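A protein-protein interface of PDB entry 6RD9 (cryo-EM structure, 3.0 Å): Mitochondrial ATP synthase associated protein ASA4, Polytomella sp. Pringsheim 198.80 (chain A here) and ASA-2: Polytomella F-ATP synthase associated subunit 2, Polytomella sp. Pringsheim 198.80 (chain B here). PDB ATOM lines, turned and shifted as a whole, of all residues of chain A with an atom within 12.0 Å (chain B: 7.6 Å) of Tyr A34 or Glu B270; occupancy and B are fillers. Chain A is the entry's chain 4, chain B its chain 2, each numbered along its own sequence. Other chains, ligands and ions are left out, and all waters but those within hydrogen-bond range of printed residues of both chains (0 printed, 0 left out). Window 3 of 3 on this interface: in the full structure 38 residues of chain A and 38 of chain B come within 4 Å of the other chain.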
ATOM      1  N   VAL A  11      14.664  21.419 -35.186  1.00  0.00           N
ATOM      2  CA  VAL A  11      14.459  21.211 -33.764  1.00  0.00           C
ATOM      3  C   VAL A  11      15.737  20.759 -33.075  1.00  0.00           C
ATOM      4  O   VAL A  11      15.828  20.834 -31.853  1.00  0.00           O
ATOM      5  CB  VAL A  11      13.301  20.223 -33.547  1.00  0.00           C
ATOM      6  CG1 VAL A  11      13.771  18.804 -33.649  1.00  0.00           C
ATOM      7  CG2 VAL A  11      12.619  20.483 -32.238  1.00  0.00           C
ATOM      8  N   ALA A  25       8.111  25.293 -30.090  1.00  0.00           N
ATOM      9  CA  ALA A  25       8.154  24.218 -31.070  1.00  0.00           C
ATOM     10  C   ALA A  25       8.990  23.056 -30.566  1.00  0.00           C
ATOM     11  O   ALA A  25       8.753  21.913 -30.959  1.00  0.00           O
ATOM     12  CB  ALA A  25       8.695  24.722 -32.402  1.00  0.00           C
ATOM     13  N   VAL A  26       9.969  23.328 -29.709  1.00  0.00           N
ATOM     14  CA  VAL A  26      10.717  22.255 -29.071  1.00  0.00           C
ATOM     15  C   VAL A  26       9.857  21.565 -28.031  1.00  0.00           C
ATOM     16  O   VAL A  26       9.814  20.333 -27.959  1.00  0.00           O
ATOM     17  CB  VAL A  26      12.008  22.814 -28.457  1.00  0.00           C
ATOM     18  CG1 VAL A  26      12.592  21.871 -27.442  1.00  0.00           C
ATOM     19  CG2 VAL A  26      12.996  23.059 -29.525  1.00  0.00           C
ATOM     20  N   LYS A  27       9.129  22.345 -27.234  1.00  0.00           N
ATOM     21  CA  LYS A  27       8.365  21.774 -26.136  1.00  0.00           C
ATOM     22  C   LYS A  27       7.167  20.979 -26.623  1.00  0.00           C
ATOM     23  O   LYS A  27       6.790  19.998 -25.986  1.00  0.00           O
ATOM     24  CB  LYS A  27       7.930  22.877 -25.181  1.00  0.00           C
ATOM     25  CG  LYS A  27       9.066  23.391 -24.322  1.00  0.00           C
ATOM     26  CD  LYS A  27       8.578  24.369 -23.284  1.00  0.00           C
ATOM     27  CE  LYS A  27       9.656  24.624 -22.255  1.00  0.00           C
ATOM     28  NZ  LYS A  27       9.127  25.389 -21.103  1.00  0.00           N
ATOM     29  N   SER A  28       6.575  21.353 -27.748  1.00  0.00           N
ATOM     30  CA  SER A  28       5.514  20.524 -28.299  1.00  0.00           C
ATOM     31  C   SER A  28       6.064  19.336 -29.072  1.00  0.00           C
ATOM     32  O   SER A  28       5.317  18.397 -29.353  1.00  0.00           O
ATOM     33  CB  SER A  28       4.595  21.343 -29.198  1.00  0.00           C
ATOM     34  OG  SER A  28       5.039  21.307 -30.536  1.00  0.00           O
ATOM     35  N   TYR A  29       7.342  19.366 -29.433  1.00  0.00           N
ATOM     36  CA  TYR A  29       7.997  18.197 -30.001  1.00  0.00           C
ATOM     37  C   TYR A  29       8.386  17.213 -28.915  1.00  0.00           C
ATOM     38  O   TYR A  29       8.234  16.004 -29.091  1.00  0.00           O
ATOM     39  CB  TYR A  29       9.227  18.626 -30.785  1.00  0.00           C
ATOM     40  CG  TYR A  29      10.027  17.510 -31.389  1.00  0.00           C
ATOM     41  CD1 TYR A  29       9.618  16.906 -32.561  1.00  0.00           C
ATOM     42  CD2 TYR A  29      11.212  17.085 -30.809  1.00  0.00           C
ATOM     43  CE1 TYR A  29      10.348  15.905 -33.125  1.00  0.00           C
ATOM     44  CE2 TYR A  29      11.946  16.080 -31.369  1.00  0.00           C
ATOM     45  CZ  TYR A  29      11.508  15.494 -32.525  1.00  0.00           C
ATOM     46  OH  TYR A  29      12.241  14.491 -33.094  1.00  0.00           O
ATOM     47  N   LEU A  30       8.876  17.713 -27.784  1.00  0.00           N
ATOM     48  CA  LEU A  30       9.232  16.842 -26.672  1.00  0.00           C
ATOM     49  C   LEU A  30       7.992  16.269 -26.002  1.00  0.00           C
ATOM     50  O   LEU A  30       8.073  15.250 -25.314  1.00  0.00           O
ATOM     51  CB  LEU A  30      10.077  17.606 -25.654  1.00  0.00           C
ATOM     52  CG  LEU A  30      11.605  17.598 -25.692  1.00  0.00           C
ATOM     53  CD1 LEU A  30      12.141  16.244 -25.404  1.00  0.00           C
ATOM     54  CD2 LEU A  30      12.116  18.045 -27.023  1.00  0.00           C
ATOM     55  N   LYS A  31       6.843  16.919 -26.171  1.00  0.00           N
ATOM     56  CA  LYS A  31       5.596  16.350 -25.681  1.00  0.00           C
ATOM     57  C   LYS A  31       5.077  15.268 -26.612  1.00  0.00           C
ATOM     58  O   LYS A  31       4.347  14.376 -26.175  1.00  0.00           O
ATOM     59  CB  LYS A  31       4.553  17.447 -25.504  1.00  0.00           C
ATOM     60  CG  LYS A  31       4.625  18.124 -24.149  1.00  0.00           C
ATOM     61  CD  LYS A  31       3.846  19.418 -24.131  1.00  0.00           C
ATOM     62  CE  LYS A  31       2.402  19.201 -24.532  1.00  0.00           C
ATOM     63  NZ  LYS A  31       1.640  20.473 -24.546  1.00  0.00           N
ATOM     64  N   SER A  32       5.425  15.335 -27.893  1.00  0.00           N
ATOM     65  CA  SER A  32       5.122  14.230 -28.792  1.00  0.00           C
ATOM     66  C   SER A  32       6.042  13.050 -28.533  1.00  0.00           C
ATOM     67  O   SER A  32       5.632  11.895 -28.665  1.00  0.00           O
ATOM     68  CB  SER A  32       5.244  14.683 -30.239  1.00  0.00           C
ATOM     69  OG  SER A  32       5.029  13.598 -31.112  1.00  0.00           O
ATOM     70  N   LEU A  33       7.292  13.315 -28.173  1.00  0.00           N
ATOM     71  CA  LEU A  33       8.203  12.229 -27.857  1.00  0.00           C
ATOM     72  C   LEU A  33       7.948  11.637 -26.485  1.00  0.00           C
ATOM     73  O   LEU A  33       8.520  10.595 -26.163  1.00  0.00           O
ATOM     74  CB  LEU A  33       9.653  12.688 -27.929  1.00  0.00           C
ATOM     75  CG  LEU A  33      10.292  13.065 -29.255  1.00  0.00           C
ATOM     76  CD1 LEU A  33      11.747  12.753 -29.140  1.00  0.00           C
ATOM     77  CD2 LEU A  33       9.682  12.326 -30.398  1.00  0.00           C
ATOM     78  N   TYR A  34       7.153  12.289 -25.647  1.00  0.00           N
ATOM     79  CA  TYR A  34       6.732  11.615 -24.429  1.00  0.00           C
ATOM     80  C   TYR A  34       5.620  10.630 -24.706  1.00  0.00           C
ATOM     81  O   TYR A  34       5.544   9.586 -24.057  1.00  0.00           O
ATOM     82  CB  TYR A  34       6.278  12.614 -23.378  1.00  0.00           C
ATOM     83  CG  TYR A  34       5.967  11.948 -22.075  1.00  0.00           C
ATOM     84  CD1 TYR A  34       4.664  11.825 -21.636  1.00  0.00           C
ATOM     85  CD2 TYR A  34       6.979  11.419 -21.296  1.00  0.00           C
ATOM     86  CE1 TYR A  34       4.378  11.212 -20.457  1.00  0.00           C
ATOM     87  CE2 TYR A  34       6.702  10.805 -20.111  1.00  0.00           C
ATOM     88  CZ  TYR A  34       5.399  10.702 -19.701  1.00  0.00           C
ATOM     89  OH  TYR A  34       5.104  10.083 -18.521  1.00  0.00           O
ATOM     90  N   ALA A  35       4.772  10.927 -25.680  1.00  0.00           N
ATOM     91  CA  ALA A  35       3.729  10.001 -26.100  1.00  0.00           C
ATOM     92  C   ALA A  35       4.225   9.078 -27.207  1.00  0.00           C
ATOM     93  O   ALA A  35       3.574   8.888 -28.233  1.00  0.00           O
ATOM     94  CB  ALA A  35       2.499  10.780 -26.541  1.00  0.00           C
ATOM     95  N   GLY A  36       5.409   8.507 -26.988  1.00  0.00           N
ATOM     96  CA  GLY A  36       5.912   7.366 -27.720  1.00  0.00           C
ATOM     97  C   GLY A  36       6.185   7.547 -29.193  1.00  0.00           C
ATOM     98  O   GLY A  36       6.380   6.543 -29.883  1.00  0.00           O
ATOM     99  N   ALA A  37       6.196   8.769 -29.712  1.00  0.00           N
ATOM    100  CA  ALA A  37       6.513   8.945 -31.120  1.00  0.00           C
ATOM    101  C   ALA A  37       7.998   8.730 -31.349  1.00  0.00           C
ATOM    102  O   ALA A  37       8.827   8.990 -30.477  1.00  0.00           O
ATOM    103  CB  ALA A  37       6.102  10.329 -31.605  1.00  0.00           C
ATOM    104  N   GLN A  38       8.331   8.210 -32.522  1.00  0.00           N
ATOM    105  CA  GLN A  38       9.707   7.829 -32.795  1.00  0.00           C
ATOM    106  C   GLN A  38      10.503   9.034 -33.265  1.00  0.00           C
ATOM    107  O   GLN A  38      10.061   9.774 -34.147  1.00  0.00           O
ATOM    108  CB  GLN A  38       9.757   6.720 -33.841  1.00  0.00           C
ATOM    109  CG  GLN A  38       9.203   5.405 -33.345  1.00  0.00           C
ATOM    110  CD  GLN A  38       9.927   4.908 -32.125  1.00  0.00           C
ATOM    111  OE1 GLN A  38       9.350   4.797 -31.049  1.00  0.00           O
ATOM    112  NE2 GLN A  38      11.205   4.606 -32.284  1.00  0.00           N
ATOM    113  N   VAL A  39      11.670   9.237 -32.662  1.00  0.00           N
ATOM    114  CA  VAL A  39      12.558  10.294 -33.117  1.00  0.00           C
ATOM    115  C   VAL A  39      13.155   9.892 -34.460  1.00  0.00           C
ATOM    116  O   VAL A  39      13.763   8.822 -34.604  1.00  0.00           O
ATOM    117  CB  VAL A  39      13.617  10.611 -32.046  1.00  0.00           C
ATOM    118  CG1 VAL A  39      14.257   9.366 -31.497  1.00  0.00           C
ATOM    119  CG2 VAL A  39      14.679  11.503 -32.603  1.00  0.00           C
ATOM    120  N   GLU A  40      12.923  10.724 -35.463  1.00  0.00           N
ATOM    121  CA  GLU A  40      13.287  10.389 -36.828  1.00  0.00           C
ATOM    122  C   GLU A  40      14.804  10.428 -36.982  1.00  0.00           C
ATOM    123  O   GLU A  40      15.490  11.240 -36.361  1.00  0.00           O
ATOM    124  CB  GLU A  40      12.590  11.361 -37.779  1.00  0.00           C
ATOM    125  CG  GLU A  40      12.305  10.853 -39.173  1.00  0.00           C
ATOM    126  CD  GLU A  40      13.541  10.777 -40.024  1.00  0.00           C
ATOM    127  OE1 GLU A  40      14.359  11.708 -39.925  1.00  0.00           O
ATOM    128  OE2 GLU A  40      13.704   9.795 -40.777  1.00  0.00           O
ATOM    129  N   VAL B 264      12.523  12.027  -7.569  1.00  0.00           N
ATOM    130  CA  VAL B 264      12.172  13.414  -7.835  1.00  0.00           C
ATOM    131  C   VAL B 264      11.870  13.611  -9.307  1.00  0.00           C
ATOM    132  O   VAL B 264      10.840  14.185  -9.673  1.00  0.00           O
ATOM    133  CB  VAL B 264      13.303  14.351  -7.389  1.00  0.00           C
ATOM    134  CG1 VAL B 264      12.896  15.774  -7.597  1.00  0.00           C
ATOM    135  CG2 VAL B 264      13.644  14.120  -5.973  1.00  0.00           C
ATOM    136  N   VAL B 265      12.755  13.123 -10.171  1.00  0.00           N
ATOM    137  CA  VAL B 265      12.731  13.551 -11.557  1.00  0.00           C
ATOM    138  C   VAL B 265      11.690  12.787 -12.349  1.00  0.00           C
ATOM    139  O   VAL B 265      11.202  13.276 -13.367  1.00  0.00           O
ATOM    140  CB  VAL B 265      14.132  13.420 -12.170  1.00  0.00           C
ATOM    141  CG1 VAL B 265      15.078  14.296 -11.431  1.00  0.00           C
ATOM    142  CG2 VAL B 265      14.608  12.024 -12.092  1.00  0.00           C
ATOM    143  N   ALA B 266      11.314  11.592 -11.904  1.00  0.00           N
ATOM    144  CA  ALA B 266      10.329  10.822 -12.664  1.00  0.00           C
ATOM    145  C   ALA B 266       8.913  11.388 -12.581  1.00  0.00           C
ATOM    146  O   ALA B 266       8.270  11.497 -13.638  1.00  0.00           O
ATOM    147  CB  ALA B 266      10.390   9.346 -12.262  1.00  0.00           C
ATOM    148  N   PRO B 267       8.358  11.774 -11.417  1.00  0.00           N
ATOM    149  CA  PRO B 267       7.028  12.397 -11.463  1.00  0.00           C
ATOM    150  C   PRO B 267       7.050  13.811 -11.995  1.00  0.00           C
ATOM    151  O   PRO B 267       5.986  14.346 -12.321  1.00  0.00           O
ATOM    152  CB  PRO B 267       6.569  12.371 -10.002  1.00  0.00           C
ATOM    153  CG  PRO B 267       7.438  11.417  -9.346  1.00  0.00           C
ATOM    154  CD  PRO B 267       8.740  11.594 -10.005  1.00  0.00           C
ATOM    155  N   ALA B 268       8.225  14.438 -12.075  1.00  0.00           N
ATOM    156  CA  ALA B 268       8.320  15.759 -12.673  1.00  0.00           C
ATOM    157  C   ALA B 268       8.254  15.683 -14.189  1.00  0.00           C
ATOM    158  O   ALA B 268       7.573  16.493 -14.825  1.00  0.00           O
ATOM    159  CB  ALA B 268       9.608  16.430 -12.228  1.00  0.00           C
ATOM    160  N   ILE B 269       8.949  14.718 -14.786  1.00  0.00           N
ATOM    161  CA  ILE B 269       8.853  14.504 -16.224  1.00  0.00           C
ATOM    162  C   ILE B 269       7.487  13.939 -16.591  1.00  0.00           C
ATOM    163  O   ILE B 269       6.933  14.258 -17.645  1.00  0.00           O
ATOM    164  CB  ILE B 269      10.008  13.595 -16.682  1.00  0.00           C
ATOM    165  CG1 ILE B 269      11.334  14.272 -16.391  1.00  0.00           C
ATOM    166  CG2 ILE B 269       9.958  13.319 -18.158  1.00  0.00           C
ATOM    167  CD1 ILE B 269      12.498  13.368 -16.511  1.00  0.00           C
ATOM    168  N   GLU B 270       6.897  13.129 -15.714  1.00  0.00           N
ATOM    169  CA  GLU B 270       5.560  12.619 -15.985  1.00  0.00           C
ATOM    170  C   GLU B 270       4.506  13.712 -15.900  1.00  0.00           C
ATOM    171  O   GLU B 270       3.469  13.622 -16.564  1.00  0.00           O
ATOM    172  CB  GLU B 270       5.222  11.487 -15.021  1.00  0.00           C
ATOM    173  CG  GLU B 270       5.877  10.182 -15.388  1.00  0.00           C
ATOM    174  CD  GLU B 270       5.418   9.029 -14.545  1.00  0.00           C
ATOM    175  OE1 GLU B 270       5.893   7.903 -14.787  1.00  0.00           O
ATOM    176  OE2 GLU B 270       4.579   9.241 -13.648  1.00  0.00           O
ATOM    177  N   LYS B 271       4.751  14.750 -15.105  1.00  0.00           N
ATOM    178  CA  LYS B 271       3.763  15.812 -14.973  1.00  0.00           C
ATOM    179  C   LYS B 271       3.873  16.801 -16.122  1.00  0.00           C
ATOM    180  O   LYS B 271       2.863  17.183 -16.720  1.00  0.00           O
ATOM    181  CB  LYS B 271       3.926  16.508 -13.626  1.00  0.00           C
ATOM    182  CG  LYS B 271       2.813  17.468 -13.269  1.00  0.00           C
ATOM    183  CD  LYS B 271       3.045  18.027 -11.881  1.00  0.00           C
ATOM    184  CE  LYS B 271       2.796  16.951 -10.831  1.00  0.00           C
ATOM    185  NZ  LYS B 271       2.903  17.456  -9.437  1.00  0.00           N
ATOM    186  N   ALA B 272       5.089  17.226 -16.442  1.00  0.00           N
ATOM    187  CA  ALA B 272       5.350  18.015 -17.635  1.00  0.00           C
ATOM    188  C   ALA B 272       6.683  17.582 -18.226  1.00  0.00           C
ATOM    189  O   ALA B 272       7.737  17.874 -17.652  1.00  0.00           O
ATOM    190  CB  ALA B 272       5.358  19.505 -17.321  1.00  0.00           C
ATOM    191  N   PRO B 273       6.675  16.879 -19.359  1.00  0.00           N
ATOM    192  CA  PRO B 273       7.932  16.363 -19.920  1.00  0.00           C
ATOM    193  C   PRO B 273       8.822  17.435 -20.496  1.00  0.00           C
ATOM    194  O   PRO B 273      10.035  17.226 -20.600  1.00  0.00           O
ATOM    195  CB  PRO B 273       7.459  15.399 -21.009  1.00  0.00           C
ATOM    196  CG  PRO B 273       5.998  15.230 -20.780  1.00  0.00           C
ATOM    197  CD  PRO B 273       5.514  16.466 -20.152  1.00  0.00           C
ATOM    198  N   ASP B 274       8.263  18.579 -20.856  1.00  0.00           N
ATOM    199  CA  ASP B 274       9.023  19.694 -21.383  1.00  0.00           C
ATOM    200  C   ASP B 274       9.549  20.618 -20.295  1.00  0.00           C
ATOM    201  O   ASP B 274       9.990  21.725 -20.601  1.00  0.00           O
ATOM    202  CB  ASP B 274       8.151  20.469 -22.359  1.00  0.00           C
ATOM    203  CG  ASP B 274       6.777  20.737 -21.812  1.00  0.00           C
ATOM    204  OD1 ASP B 274       6.489  20.269 -20.696  1.00  0.00           O
ATOM    205  OD2 ASP B 274       5.973  21.403 -22.493  1.00  0.00           O
ATOM    206  N   LEU B 295      13.958   3.494 -14.577  1.00  0.00           N
ATOM    207  CA  LEU B 295      13.011   4.596 -14.493  1.00  0.00           C
ATOM    208  C   LEU B 295      11.633   4.055 -14.822  1.00  0.00           C
ATOM    209  O   LEU B 295      11.496   2.885 -15.191  1.00  0.00           O
ATOM    210  CB  LEU B 295      13.416   5.699 -15.487  1.00  0.00           C
ATOM    211  CG  LEU B 295      14.742   6.424 -15.285  1.00  0.00           C
ATOM    212  CD1 LEU B 295      14.973   7.315 -16.470  1.00  0.00           C
ATOM    213  CD2 LEU B 295      14.731   7.226 -14.002  1.00  0.00           C
ATOM    214  N   PRO B 296      10.579   4.864 -14.673  1.00  0.00           N
ATOM    215  CA  PRO B 296       9.267   4.468 -15.199  1.00  0.00           C
ATOM    216  C   PRO B 296       9.262   4.195 -16.697  1.00  0.00           C
ATOM    217  O   PRO B 296      10.164   4.582 -17.439  1.00  0.00           O
ATOM    218  CB  PRO B 296       8.383   5.665 -14.854  1.00  0.00           C
ATOM    219  CG  PRO B 296       8.932   6.131 -13.581  1.00  0.00           C
ATOM    220  CD  PRO B 296      10.416   5.865 -13.604  1.00  0.00           C
ATOM    221  N   ALA B 297       8.222   3.485 -17.130  1.00  0.00           N
ATOM    222  CA  ALA B 297       8.192   2.967 -18.491  1.00  0.00           C
ATOM    223  C   ALA B 297       7.966   4.069 -19.509  1.00  0.00           C
ATOM    224  O   ALA B 297       8.407   3.951 -20.656  1.00  0.00           O
ATOM    225  CB  ALA B 297       7.110   1.899 -18.624  1.00  0.00           C
ATOM    226  N   ALA B 298       7.286   5.138 -19.119  1.00  0.00           N
ATOM    227  CA  ALA B 298       7.100   6.266 -20.012  1.00  0.00           C
ATOM    228  C   ALA B 298       8.236   7.265 -19.928  1.00  0.00           C
ATOM    229  O   ALA B 298       8.342   8.121 -20.804  1.00  0.00           O
ATOM    230  CB  ALA B 298       5.776   6.973 -19.714  1.00  0.00           C
ATOM    231  N   VAL B 299       9.085   7.172 -18.914  1.00  0.00           N
ATOM    232  CA  VAL B 299      10.163   8.124 -18.706  1.00  0.00           C
ATOM    233  C   VAL B 299      11.459   7.638 -19.325  1.00  0.00           C
ATOM    234  O   VAL B 299      12.080   8.354 -20.108  1.00  0.00           O
ATOM    235  CB  VAL B 299      10.334   8.414 -17.199  1.00  0.00           C
ATOM    236  CG1 VAL B 299      11.647   9.105 -16.924  1.00  0.00           C
ATOM    237  CG2 VAL B 299       9.213   9.263 -16.717  1.00  0.00           C
ATOM    238  N   GLY B 300      11.874   6.412 -18.999  1.00  0.00           N
ATOM    239  CA  GLY B 300      13.151   5.909 -19.477  1.00  0.00           C
ATOM    240  C   GLY B 300      13.178   5.650 -20.966  1.00  0.00           C
ATOM    241  O   GLY B 300      14.247   5.661 -21.580  1.00  0.00           O
ATOM    242  N   SER B 301      12.016   5.407 -21.566  1.00  0.00           N
ATOM    243  CA  SER B 301      11.943   5.365 -23.018  1.00  0.00           C
ATOM    244  C   SER B 301      11.951   6.758 -23.612  1.00  0.00           C
ATOM    245  O   SER B 301      12.373   6.937 -24.756  1.00  0.00           O
ATOM    246  CB  SER B 301      10.692   4.626 -23.467  1.00  0.00           C
ATOM    247  OG  SER B 301      10.575   4.667 -24.877  1.00  0.00           O
ATOM    248  N   PHE B 302      11.487   7.751 -22.856  1.00  0.00           N
ATOM    249  CA  PHE B 302      11.452   9.122 -23.346  1.00  0.00           C
ATOM    250  C   PHE B 302      12.809   9.794 -23.227  1.00  0.00           C
ATOM    251  O   PHE B 302      13.219  10.516 -24.135  1.00  0.00           O
ATOM    252  CB  PHE B 302      10.388   9.910 -22.591  1.00  0.00           C
ATOM    253  CG  PHE B 302      10.528  11.392 -22.698  1.00  0.00           C
ATOM    254  CD1 PHE B 302      10.885  12.140 -21.597  1.00  0.00           C
ATOM    255  CD2 PHE B 302      10.276  12.041 -23.887  1.00  0.00           C
ATOM    256  CE1 PHE B 302      11.009  13.493 -21.686  1.00  0.00           C
ATOM    257  CE2 PHE B 302      10.393  13.404 -23.971  1.00  0.00           C
ATOM    258  CZ  PHE B 302      10.758  14.123 -22.870  1.00  0.00           C
ATOM    259  N   VAL B 303      13.533   9.566 -22.130  1.00  0.00           N
ATOM    260  CA  VAL B 303      14.875  10.130 -22.038  1.00  0.00           C
ATOM    261  C   VAL B 303      15.883   9.360 -22.866  1.00  0.00           C
ATOM    262  O   VAL B 303      17.024   9.806 -23.000  1.00  0.00           O
ATOM    263  CB  VAL B 303      15.379  10.205 -20.588  1.00  0.00           C
ATOM    264  CG1 VAL B 303      14.318  10.795 -19.721  1.00  0.00           C
ATOM    265  CG2 VAL B 303      15.797   8.849 -20.091  1.00  0.00           C
ATOM    266  N   LYS B 305      15.272   8.771 -26.103  1.00  0.00           N
ATOM    267  CA  LYS B 305      15.265   9.550 -27.328  1.00  0.00           C
ATOM    268  C   LYS B 305      15.996  10.864 -27.128  1.00  0.00           C
ATOM    269  O   LYS B 305      16.671  11.348 -28.038  1.00  0.00           O
ATOM    270  CB  LYS B 305      13.836   9.802 -27.779  1.00  0.00           C
ATOM    271  CG  LYS B 305      12.916   8.645 -27.554  1.00  0.00           C
ATOM    272  CD  LYS B 305      11.576   8.908 -28.178  1.00  0.00           C
ATOM    273  CE  LYS B 305      10.575   7.879 -27.748  1.00  0.00           C
ATOM    274  NZ  LYS B 305       9.239   8.209 -28.268  1.00  0.00           N
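The backbone NH (N) of Ala A37 sits at hydrogen-bond distance from the backbone carbonyl oxygen (O) of Ser A32 (3.3 Å).
Hydrophobic or aromatic side chains of chain B that line the printed part of chain A: Pro B273, Ala B298 and Phe B302.
Among the printed residues, 12 pairs touch across the chains.
Among the printed residues, no Asp or Glu carboxylate lies within 4 Å of a Lys or Arg side-chain nitrogen of the other chain.
The side-chain amino group (NZ) of Lys B305 sits at hydrogen-bond distance from the backbone carbonyl oxygen (O) of Leu A33 (3.3 Å).
The side-chain amino group (NZ) of Lys B305 lies close to the backbone carbonyl oxygen (O) of Ala A37.
Printed residues of chain B within 4 Å of Lys A27: Asp B274 (3.4 Å).
Tyr A29 touches none of the printed residues of chain B.
Of the printed residues of chain B, Leu A30 touches Phe B302 (3.3 Å).
Of chain B, only Glu B270, Pro B273, Ala B298 and Phe B302 come within 4 Å of Tyr A34.
Printed residues of chain B within 4 Å of Ala A37: Lys B305 (2.4 Å).
Printed residues of chain B within 4 Å of Val A39: Lys B305 (3.8 Å).
No residue of chain A comes within 4 Å of Ala B268.
No residue of chain A comes within 4 Å of Ile B269.
Glu B270 touches one residue of chain A.
No residue of chain A comes within 4 Å of Lys B271.
No residue of chain A comes within 4 Å of Ala B272.
Of the printed residues of chain A, Pro B273 touches Tyr A34.
Of the printed residues of chain A, Asp B274 touches Lys A27 (3.4 Å) and Lys A31 (3.3 Å).
Of chain A, only Tyr A34 (3.2 Å) comes within 4 Å of Ala B298.
No residue of chain A comes within 4 Å of Val B299.
Phe B302 touches three residues of chain A.
The nearest residue of chain B that does not touch Tyr A34 is Ile B269 (4.2 Å).
The nearest printed residue of chain B that does not touch Lys A31 is Pro B273 (4.4 Å).
Lys A27 touches Asp B274 (CE to O, 3.4 Å).
Leu A30 touches Phe B302 (O to CE2, 3.3 Å).
Lys A31 touches Asp B274.
CD2 of Phe B302 touches O of Leu A33 (3.2 Å).
CG of Glu B270 touches OH of Tyr A34, 3.2 Å away.
CG of Pro B273 touches CG of Tyr A34, 3.5 Å away.
CE2 of Tyr A34 touches O of Ala B298 (3.2 Å).
N of Tyr A34 touches CD2 of Phe B302 (3.6 Å).
Lys B305 touches Gly A36.
Lys B305 touches Val A39.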
